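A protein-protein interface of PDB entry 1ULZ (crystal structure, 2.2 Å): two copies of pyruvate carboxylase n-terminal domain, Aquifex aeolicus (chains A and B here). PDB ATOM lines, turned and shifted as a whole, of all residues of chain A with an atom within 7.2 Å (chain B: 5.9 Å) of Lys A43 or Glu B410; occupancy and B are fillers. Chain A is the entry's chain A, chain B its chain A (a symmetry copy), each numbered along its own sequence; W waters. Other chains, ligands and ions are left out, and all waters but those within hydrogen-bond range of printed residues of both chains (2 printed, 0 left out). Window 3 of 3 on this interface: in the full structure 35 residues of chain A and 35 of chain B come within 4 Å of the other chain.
Water W2 bridges NH2 of Arg A40 (2.7 Å) and O of Thr B408 (3.0 Å). Water W1 bridges N of Arg A373 (2.8 Å) and O of Tyr B357 (2.9 Å).
Printed residues of chain B within 4 Å of Arg A40: Tyr B358 (3.4 Å) and Glu B410 (2.5 Å). Of the printed residues of chain B, Lys A43 touches Glu B410. Printed residues of chain B within 4 Å of Leu A44: Thr B408. Ala A45 touches none of the printed residues of chain B. Of the printed residues of chain B, Ala A372 touches Tyr B357 (3.7 Å). Of the printed residues of chain A, Tyr B357 touches Ala A372. Of the printed residues of chain A, Thr B408 touches Leu A44 (3.8 Å). Glu B410 touches two residues of chain A. Thr B412 touches none of the printed residues of chain A. The nearest residue of chain B that does not touch Lys A43 is Arg B356 (4.8 Å).
The guanidinium group of Arg A40 is in salt-bridge range of the side-chain carboxylate of Glu B410 (2.5 Å). NZ of Lys A43 is in salt-bridge range of OE2 of Glu B410, 3.6 Å away.
Arg A40 touches Tyr B358 (CD to CD2, 3.4 Å). Thr B408 touches Leu A44 (CB to CD2, 3.8 Å). Ala A372 touches Tyr B357 (CB to O, 3.7 Å).
No position is printed for both chains. Of the 5 pairs that touch across the chains among the printed residues, none has its exchanged pair printed and touching as well.
Of the 12 printed residues of chain B, 4 touch a printed residue of chain A. Of the 15 printed residues of chain A, 4 touch a printed residue of chain B.
The guanidinium group of Arg B356 is in salt-bridge range of the side-chain carboxylate of Glu B410 (2.7 Å). OH of Tyr B357 lies within hydrogen-bond range of OH of Tyr B409, at 2.8 Å. The backbone NH (N) of Tyr B358 lies within hydrogen-bond range of the backbone carbonyl oxygen (O) of Glu B410.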
ATOM      1  N   ILE A  18       3.013   0.905  25.680  1.00  0.00           N
ATOM      2  CA  ILE A  18       1.777   0.163  25.913  1.00  0.00           C
ATOM      3  C   ILE A  18       1.374   0.209  27.390  1.00  0.00           C
ATOM      4  O   ILE A  18       0.200   0.375  27.708  1.00  0.00           O
ATOM      5  CB  ILE A  18       1.903  -1.315  25.456  1.00  0.00           C
ATOM      6  CG1 ILE A  18       1.845  -1.391  23.928  1.00  0.00           C
ATOM      7  CG2 ILE A  18       0.781  -2.154  26.053  1.00  0.00           C
ATOM      8  CD1 ILE A  18       2.074  -2.778  23.377  1.00  0.00           C
ATOM      9  N   ALA A  30      -0.708  -2.636  18.069  1.00  0.00           N
ATOM     10  CA  ALA A  30       0.684  -2.962  17.801  1.00  0.00           C
ATOM     11  C   ALA A  30       0.896  -3.398  16.353  1.00  0.00           C
ATOM     12  O   ALA A  30      -0.011  -3.931  15.717  1.00  0.00           O
ATOM     13  CB  ALA A  30       1.142  -4.076  18.743  1.00  0.00           C
ATOM     14  N   SER A  37       6.673 -12.427  15.388  1.00  0.00           N
ATOM     15  CA  SER A  37       5.269 -12.707  15.652  1.00  0.00           C
ATOM     16  C   SER A  37       5.010 -13.084  17.108  1.00  0.00           C
ATOM     17  O   SER A  37       3.863 -13.068  17.550  1.00  0.00           O
ATOM     18  CB  SER A  37       4.757 -13.823  14.734  1.00  0.00           C
ATOM     19  OG  SER A  37       5.492 -15.021  14.898  1.00  0.00           O
ATOM     20  N   THR A  38       6.066 -13.427  17.845  1.00  0.00           N
ATOM     21  CA  THR A  38       5.914 -13.793  19.250  1.00  0.00           C
ATOM     22  C   THR A  38       6.505 -12.733  20.175  1.00  0.00           C
ATOM     23  O   THR A  38       6.695 -12.977  21.363  1.00  0.00           O
ATOM     24  CB  THR A  38       6.587 -15.167  19.578  1.00  0.00           C
ATOM     25  OG1 THR A  38       7.990 -15.112  19.283  1.00  0.00           O
ATOM     26  CG2 THR A  38       5.953 -16.278  18.762  1.00  0.00           C
ATOM     27  N   ALA A  39       6.799 -11.557  19.628  1.00  0.00           N
ATOM     28  CA  ALA A  39       7.368 -10.477  20.425  1.00  0.00           C
ATOM     29  C   ALA A  39       6.424 -10.082  21.555  1.00  0.00           C
ATOM     30  O   ALA A  39       5.213 -10.280  21.464  1.00  0.00           O
ATOM     31  CB  ALA A  39       7.659  -9.271  19.540  1.00  0.00           C
ATOM     32  N   ARG A  40       6.989  -9.506  22.611  1.00  0.00           N
ATOM     33  CA  ARG A  40       6.214  -9.091  23.776  1.00  0.00           C
ATOM     34  C   ARG A  40       5.124  -8.063  23.498  1.00  0.00           C
ATOM     35  O   ARG A  40       3.979  -8.251  23.913  1.00  0.00           O
ATOM     36  CB  ARG A  40       7.132  -8.522  24.856  1.00  0.00           C
ATOM     37  CG  ARG A  40       6.597  -8.715  26.263  1.00  0.00           C
ATOM     38  CD  ARG A  40       6.928 -10.123  26.716  1.00  0.00           C
ATOM     39  NE  ARG A  40       5.747 -10.885  27.083  1.00  0.00           N
ATOM     40  CZ  ARG A  40       5.754 -12.199  27.277  1.00  0.00           C
ATOM     41  NH1 ARG A  40       6.878 -12.887  27.132  1.00  0.00           N
ATOM     42  NH2 ARG A  40       4.639 -12.822  27.620  1.00  0.00           N
ATOM     43  N   HIS A  41       5.468  -6.974  22.810  1.00  0.00           N
ATOM     44  CA  HIS A  41       4.468  -5.941  22.550  1.00  0.00           C
ATOM     45  C   HIS A  41       3.264  -6.459  21.778  1.00  0.00           C
ATOM     46  O   HIS A  41       2.145  -5.991  21.974  1.00  0.00           O
ATOM     47  CB  HIS A  41       5.088  -4.719  21.844  1.00  0.00           C
ATOM     48  CG  HIS A  41       5.507  -4.965  20.428  1.00  0.00           C
ATOM     49  ND1 HIS A  41       6.632  -5.690  20.097  1.00  0.00           N
ATOM     50  CD2 HIS A  41       4.963  -4.555  19.257  1.00  0.00           C
ATOM     51  CE1 HIS A  41       6.764  -5.714  18.782  1.00  0.00           C
ATOM     52  NE2 HIS A  41       5.764  -5.032  18.248  1.00  0.00           N
ATOM     53  N   VAL A  42       3.494  -7.440  20.915  1.00  0.00           N
ATOM     54  CA  VAL A  42       2.422  -8.040  20.136  1.00  0.00           C
ATOM     55  C   VAL A  42       1.392  -8.671  21.071  1.00  0.00           C
ATOM     56  O   VAL A  42       0.186  -8.514  20.873  1.00  0.00           O
ATOM     57  CB  VAL A  42       2.953  -9.141  19.205  1.00  0.00           C
ATOM     58  CG1 VAL A  42       1.785  -9.871  18.573  1.00  0.00           C
ATOM     59  CG2 VAL A  42       3.871  -8.538  18.138  1.00  0.00           C
ATOM     60  N   LYS A  43       1.878  -9.380  22.089  1.00  0.00           N
ATOM     61  CA  LYS A  43       1.010 -10.042  23.066  1.00  0.00           C
ATOM     62  C   LYS A  43       0.311  -9.059  23.999  1.00  0.00           C
ATOM     63  O   LYS A  43      -0.854  -9.246  24.351  1.00  0.00           O
ATOM     64  CB  LYS A  43       1.817 -11.008  23.942  1.00  0.00           C
ATOM     65  CG  LYS A  43       2.568 -12.096  23.203  1.00  0.00           C
ATOM     66  CD  LYS A  43       3.378 -12.942  24.189  1.00  0.00           C
ATOM     67  CE  LYS A  43       4.141 -14.054  23.485  1.00  0.00           C
ATOM     68  NZ  LYS A  43       4.984 -14.801  24.462  1.00  0.00           N
ATOM     69  N   LEU A  44       1.031  -8.021  24.416  1.00  0.00           N
ATOM     70  CA  LEU A  44       0.480  -7.042  25.345  1.00  0.00           C
ATOM     71  C   LEU A  44      -0.546  -6.076  24.760  1.00  0.00           C
ATOM     72  O   LEU A  44      -1.398  -5.566  25.488  1.00  0.00           O
ATOM     73  CB  LEU A  44       1.610  -6.249  26.003  1.00  0.00           C
ATOM     74  CG  LEU A  44       2.667  -7.073  26.746  1.00  0.00           C
ATOM     75  CD1 LEU A  44       3.498  -6.142  27.616  1.00  0.00           C
ATOM     76  CD2 LEU A  44       2.003  -8.142  27.604  1.00  0.00           C
ATOM     77  N   ALA A  45      -0.478  -5.826  23.456  1.00  0.00           N
ATOM     78  CA  ALA A  45      -1.419  -4.905  22.821  1.00  0.00           C
ATOM     79  C   ALA A  45      -2.835  -5.479  22.720  1.00  0.00           C
ATOM     80  O   ALA A  45      -3.023  -6.699  22.725  1.00  0.00           O
ATOM     81  CB  ALA A  45      -0.915  -4.522  21.438  1.00  0.00           C
ATOM     82  N   ASP A  46      -3.828  -4.596  22.639  1.00  0.00           N
ATOM     83  CA  ASP A  46      -5.224  -5.020  22.516  1.00  0.00           C
ATOM     84  C   ASP A  46      -5.478  -5.517  21.092  1.00  0.00           C
ATOM     85  O   ASP A  46      -6.261  -6.436  20.879  1.00  0.00           O
ATOM     86  CB  ASP A  46      -6.175  -3.861  22.842  1.00  0.00           C
ATOM     87  CG  ASP A  46      -5.907  -3.257  24.210  1.00  0.00           C
ATOM     88  OD1 ASP A  46      -5.433  -2.105  24.271  1.00  0.00           O
ATOM     89  OD2 ASP A  46      -6.158  -3.941  25.228  1.00  0.00           O
ATOM     90  N   ALA A  48      -3.171  -6.193  17.274  1.00  0.00           N
ATOM     91  CA  ALA A  48      -1.816  -6.320  16.748  1.00  0.00           C
ATOM     92  C   ALA A  48      -1.858  -6.780  15.292  1.00  0.00           C
ATOM     93  O   ALA A  48      -2.536  -7.752  14.956  1.00  0.00           O
ATOM     94  CB  ALA A  48      -1.010  -7.303  17.604  1.00  0.00           C
ATOM     95  N   ALA A 372      12.359 -12.862  27.784  1.00  0.00           N
ATOM     96  CA  ALA A 372      11.987 -14.050  28.543  1.00  0.00           C
ATOM     97  C   ALA A 372      12.685 -15.203  27.830  1.00  0.00           C
ATOM     98  O   ALA A 372      13.340 -14.992  26.809  1.00  0.00           O
ATOM     99  CB  ALA A 372      10.475 -14.251  28.512  1.00  0.00           C
ATOM    100  N   ARG A 373      12.571 -16.411  28.368  1.00  0.00           N
ATOM    101  CA  ARG A 373      13.181 -17.553  27.710  1.00  0.00           C
ATOM    102  C   ARG A 373      12.571 -17.621  26.315  1.00  0.00           C
ATOM    103  O   ARG A 373      11.363 -17.462  26.155  1.00  0.00           O
ATOM    104  CB  ARG A 373      12.870 -18.843  28.462  1.00  0.00           C
ATOM    105  CG  ARG A 373      13.384 -20.076  27.741  1.00  0.00           C
ATOM    106  CD  ARG A 373      13.407 -21.295  28.642  1.00  0.00           C
ATOM    107  NE  ARG A 373      13.995 -22.444  27.954  1.00  0.00           N
ATOM    108  CZ  ARG A 373      13.440 -23.054  26.912  1.00  0.00           C
ATOM    109  NH1 ARG A 373      12.268 -22.632  26.440  1.00  0.00           N
ATOM    110  NH2 ARG A 373      14.063 -24.074  26.328  1.00  0.00           N
ATOM    111  N   ARG B 356       6.080 -20.819  30.674  1.00  0.00           N
ATOM    112  CA  ARG B 356       6.323 -19.452  30.222  1.00  0.00           C
ATOM    113  C   ARG B 356       6.320 -18.555  31.456  1.00  0.00           C
ATOM    114  O   ARG B 356       5.575 -18.790  32.407  1.00  0.00           O
ATOM    115  CB  ARG B 356       5.270 -19.019  29.195  1.00  0.00           C
ATOM    116  CG  ARG B 356       5.189 -20.001  28.026  1.00  0.00           C
ATOM    117  CD  ARG B 356       4.725 -19.386  26.709  1.00  0.00           C
ATOM    118  NE  ARG B 356       3.330 -18.964  26.726  1.00  0.00           N
ATOM    119  CZ  ARG B 356       2.567 -18.860  25.637  1.00  0.00           C
ATOM    120  NH1 ARG B 356       3.061 -19.157  24.437  1.00  0.00           N
ATOM    121  NH2 ARG B 356       1.303 -18.455  25.743  1.00  0.00           N
ATOM    122  N   TYR B 357       7.184 -17.549  31.459  1.00  0.00           N
ATOM    123  CA  TYR B 357       7.287 -16.655  32.603  1.00  0.00           C
ATOM    124  C   TYR B 357       7.851 -15.303  32.188  1.00  0.00           C
ATOM    125  O   TYR B 357       9.022 -15.198  31.826  1.00  0.00           O
ATOM    126  CB  TYR B 357       8.189 -17.296  33.676  1.00  0.00           C
ATOM    127  CG  TYR B 357       8.216 -16.563  35.009  1.00  0.00           C
ATOM    128  CD1 TYR B 357       9.359 -15.892  35.436  1.00  0.00           C
ATOM    129  CD2 TYR B 357       7.095 -16.527  35.827  1.00  0.00           C
ATOM    130  CE1 TYR B 357       9.378 -15.210  36.631  1.00  0.00           C
ATOM    131  CE2 TYR B 357       7.104 -15.843  37.029  1.00  0.00           C
ATOM    132  CZ  TYR B 357       8.245 -15.185  37.425  1.00  0.00           C
ATOM    133  OH  TYR B 357       8.244 -14.475  38.608  1.00  0.00           O
ATOM    134  N   TYR B 358       7.001 -14.276  32.213  1.00  0.00           N
ATOM    135  CA  TYR B 358       7.429 -12.925  31.871  1.00  0.00           C
ATOM    136  C   TYR B 358       7.081 -11.986  33.018  1.00  0.00           C
ATOM    137  O   TYR B 358       5.925 -11.878  33.429  1.00  0.00           O
ATOM    138  CB  TYR B 358       6.780 -12.437  30.569  1.00  0.00           C
ATOM    139  CG  TYR B 358       7.072 -10.980  30.284  1.00  0.00           C
ATOM    140  CD1 TYR B 358       6.149  -9.989  30.608  1.00  0.00           C
ATOM    141  CD2 TYR B 358       8.297 -10.586  29.751  1.00  0.00           C
ATOM    142  CE1 TYR B 358       6.433  -8.650  30.413  1.00  0.00           C
ATOM    143  CE2 TYR B 358       8.596  -9.249  29.556  1.00  0.00           C
ATOM    144  CZ  TYR B 358       7.659  -8.282  29.891  1.00  0.00           C
ATOM    145  OH  TYR B 358       7.961  -6.949  29.736  1.00  0.00           O
ATOM    146  N   VAL B 359       8.100 -11.308  33.526  1.00  0.00           N
ATOM    147  CA  VAL B 359       7.951 -10.392  34.646  1.00  0.00           C
ATOM    148  C   VAL B 359       7.743  -8.959  34.179  1.00  0.00           C
ATOM    149  O   VAL B 359       8.542  -8.421  33.416  1.00  0.00           O
ATOM    150  CB  VAL B 359       9.210 -10.433  35.549  1.00  0.00           C
ATOM    151  CG1 VAL B 359       9.004  -9.560  36.774  1.00  0.00           C
ATOM    152  CG2 VAL B 359       9.512 -11.864  35.957  1.00  0.00           C
ATOM    153  N   PRO B 360       6.649  -8.325  34.624  1.00  0.00           N
ATOM    154  CA  PRO B 360       6.369  -6.941  34.233  1.00  0.00           C
ATOM    155  C   PRO B 360       7.318  -5.979  34.926  1.00  0.00           C
ATOM    156  O   PRO B 360       7.809  -6.262  36.025  1.00  0.00           O
ATOM    157  CB  PRO B 360       4.920  -6.741  34.668  1.00  0.00           C
ATOM    158  CG  PRO B 360       4.799  -7.641  35.862  1.00  0.00           C
ATOM    159  CD  PRO B 360       5.536  -8.892  35.404  1.00  0.00           C
ATOM    160  N   LEU B 406      -0.489  -6.733  36.325  1.00  0.00           N
ATOM    161  CA  LEU B 406      -1.045  -8.085  36.388  1.00  0.00           C
ATOM    162  C   LEU B 406      -1.444  -8.601  35.005  1.00  0.00           C
ATOM    163  O   LEU B 406      -1.191  -9.753  34.679  1.00  0.00           O
ATOM    164  CB  LEU B 406      -2.266  -8.119  37.319  1.00  0.00           C
ATOM    165  CG  LEU B 406      -1.980  -7.969  38.822  1.00  0.00           C
ATOM    166  CD1 LEU B 406      -3.280  -7.763  39.593  1.00  0.00           C
ATOM    167  CD2 LEU B 406      -1.247  -9.199  39.322  1.00  0.00           C
ATOM    168  N   THR B 408      -0.110  -8.006  32.299  1.00  0.00           N
ATOM    169  CA  THR B 408       1.060  -8.278  31.469  1.00  0.00           C
ATOM    170  C   THR B 408       1.967  -9.355  32.057  1.00  0.00           C
ATOM    171  O   THR B 408       3.016  -9.657  31.496  1.00  0.00           O
ATOM    172  CB  THR B 408       1.915  -7.011  31.265  1.00  0.00           C
ATOM    173  OG1 THR B 408       2.446  -6.583  32.527  1.00  0.00           O
ATOM    174  CG2 THR B 408       1.082  -5.894  30.663  1.00  0.00           C
ATOM    175  N   TYR B 409       1.558  -9.934  33.183  1.00  0.00           N
ATOM    176  CA  TYR B 409       2.353 -10.962  33.857  1.00  0.00           C
ATOM    177  C   TYR B 409       2.029 -12.343  33.301  1.00  0.00           C
ATOM    178  O   TYR B 409       1.019 -12.941  33.672  1.00  0.00           O
ATOM    179  CB  TYR B 409       2.059 -10.925  35.359  1.00  0.00           C
ATOM    180  CG  TYR B 409       3.198 -11.342  36.274  1.00  0.00           C
ATOM    181  CD1 TYR B 409       3.332 -10.767  37.535  1.00  0.00           C
ATOM    182  CD2 TYR B 409       4.124 -12.301  35.893  1.00  0.00           C
ATOM    183  CE1 TYR B 409       4.355 -11.129  38.389  1.00  0.00           C
ATOM    184  CE2 TYR B 409       5.160 -12.677  36.750  1.00  0.00           C
ATOM    185  CZ  TYR B 409       5.267 -12.080  37.996  1.00  0.00           C
ATOM    186  OH  TYR B 409       6.286 -12.422  38.852  1.00  0.00           O
ATOM    187  N   GLU B 410       2.878 -12.856  32.416  1.00  0.00           N
ATOM    188  CA  GLU B 410       2.621 -14.176  31.849  1.00  0.00           C
ATOM    189  C   GLU B 410       3.237 -15.300  32.682  1.00  0.00           C
ATOM    190  O   GLU B 410       4.409 -15.252  33.043  1.00  0.00           O
ATOM    191  CB  GLU B 410       3.155 -14.286  30.416  1.00  0.00           C
ATOM    192  CG  GLU B 410       2.692 -15.576  29.734  1.00  0.00           C
ATOM    193  CD  GLU B 410       3.233 -15.769  28.324  1.00  0.00           C
ATOM    194  OE1 GLU B 410       2.561 -16.455  27.528  1.00  0.00           O
ATOM    195  OE2 GLU B 410       4.324 -15.260  28.008  1.00  0.00           O
ATOM    196  N   ILE B 411       2.426 -16.304  32.987  1.00  0.00           N
ATOM    197  CA  ILE B 411       2.866 -17.468  33.747  1.00  0.00           C
ATOM    198  C   ILE B 411       2.044 -18.674  33.288  1.00  0.00           C
ATOM    199  O   ILE B 411       0.816 -18.656  33.386  1.00  0.00           O
ATOM    200  CB  ILE B 411       2.627 -17.299  35.270  1.00  0.00           C
ATOM    201  CG1 ILE B 411       3.412 -16.106  35.812  1.00  0.00           C
ATOM    202  CG2 ILE B 411       3.033 -18.569  35.998  1.00  0.00           C
ATOM    203  CD1 ILE B 411       3.308 -15.945  37.316  1.00  0.00           C
ATOM    204  N   THR B 412       2.708 -19.704  32.769  1.00  0.00           N
ATOM    205  CA  THR B 412       2.003 -20.914  32.346  1.00  0.00           C
ATOM    206  C   THR B 412       2.648 -22.139  32.984  1.00  0.00           C
ATOM    207  O   THR B 412       3.778 -22.076  33.470  1.00  0.00           O
ATOM    208  CB  THR B 412       2.003 -21.101  30.804  1.00  0.00           C
ATOM    209  OG1 THR B 412       3.346 -21.271  30.334  1.00  0.00           O
ATOM    210  CG2 THR B 412       1.366 -19.900  30.123  1.00  0.00           C
ATOM    211  N   ILE B 418      -3.499 -14.723  39.526  1.00  0.00           N
ATOM    212  CA  ILE B 418      -3.549 -13.550  38.656  1.00  0.00           C
ATOM    213  C   ILE B 418      -4.937 -13.184  38.121  1.00  0.00           C
ATOM    214  O   ILE B 418      -5.326 -12.019  38.160  1.00  0.00           O
ATOM    215  CB  ILE B 418      -2.550 -13.689  37.483  1.00  0.00           C
ATOM    216  CG1 ILE B 418      -1.119 -13.597  38.024  1.00  0.00           C
ATOM    217  CG2 ILE B 418      -2.796 -12.603  36.444  1.00  0.00           C
ATOM    218  CD1 ILE B 418      -0.048 -13.844  36.991  1.00  0.00           C
HETATM  219  O   HOH W   1      11.095 -16.801  30.664  1.00  0.00           O
HETATM  220  O   HOH W   2       3.018 -11.020  28.828  1.00  0.00           O
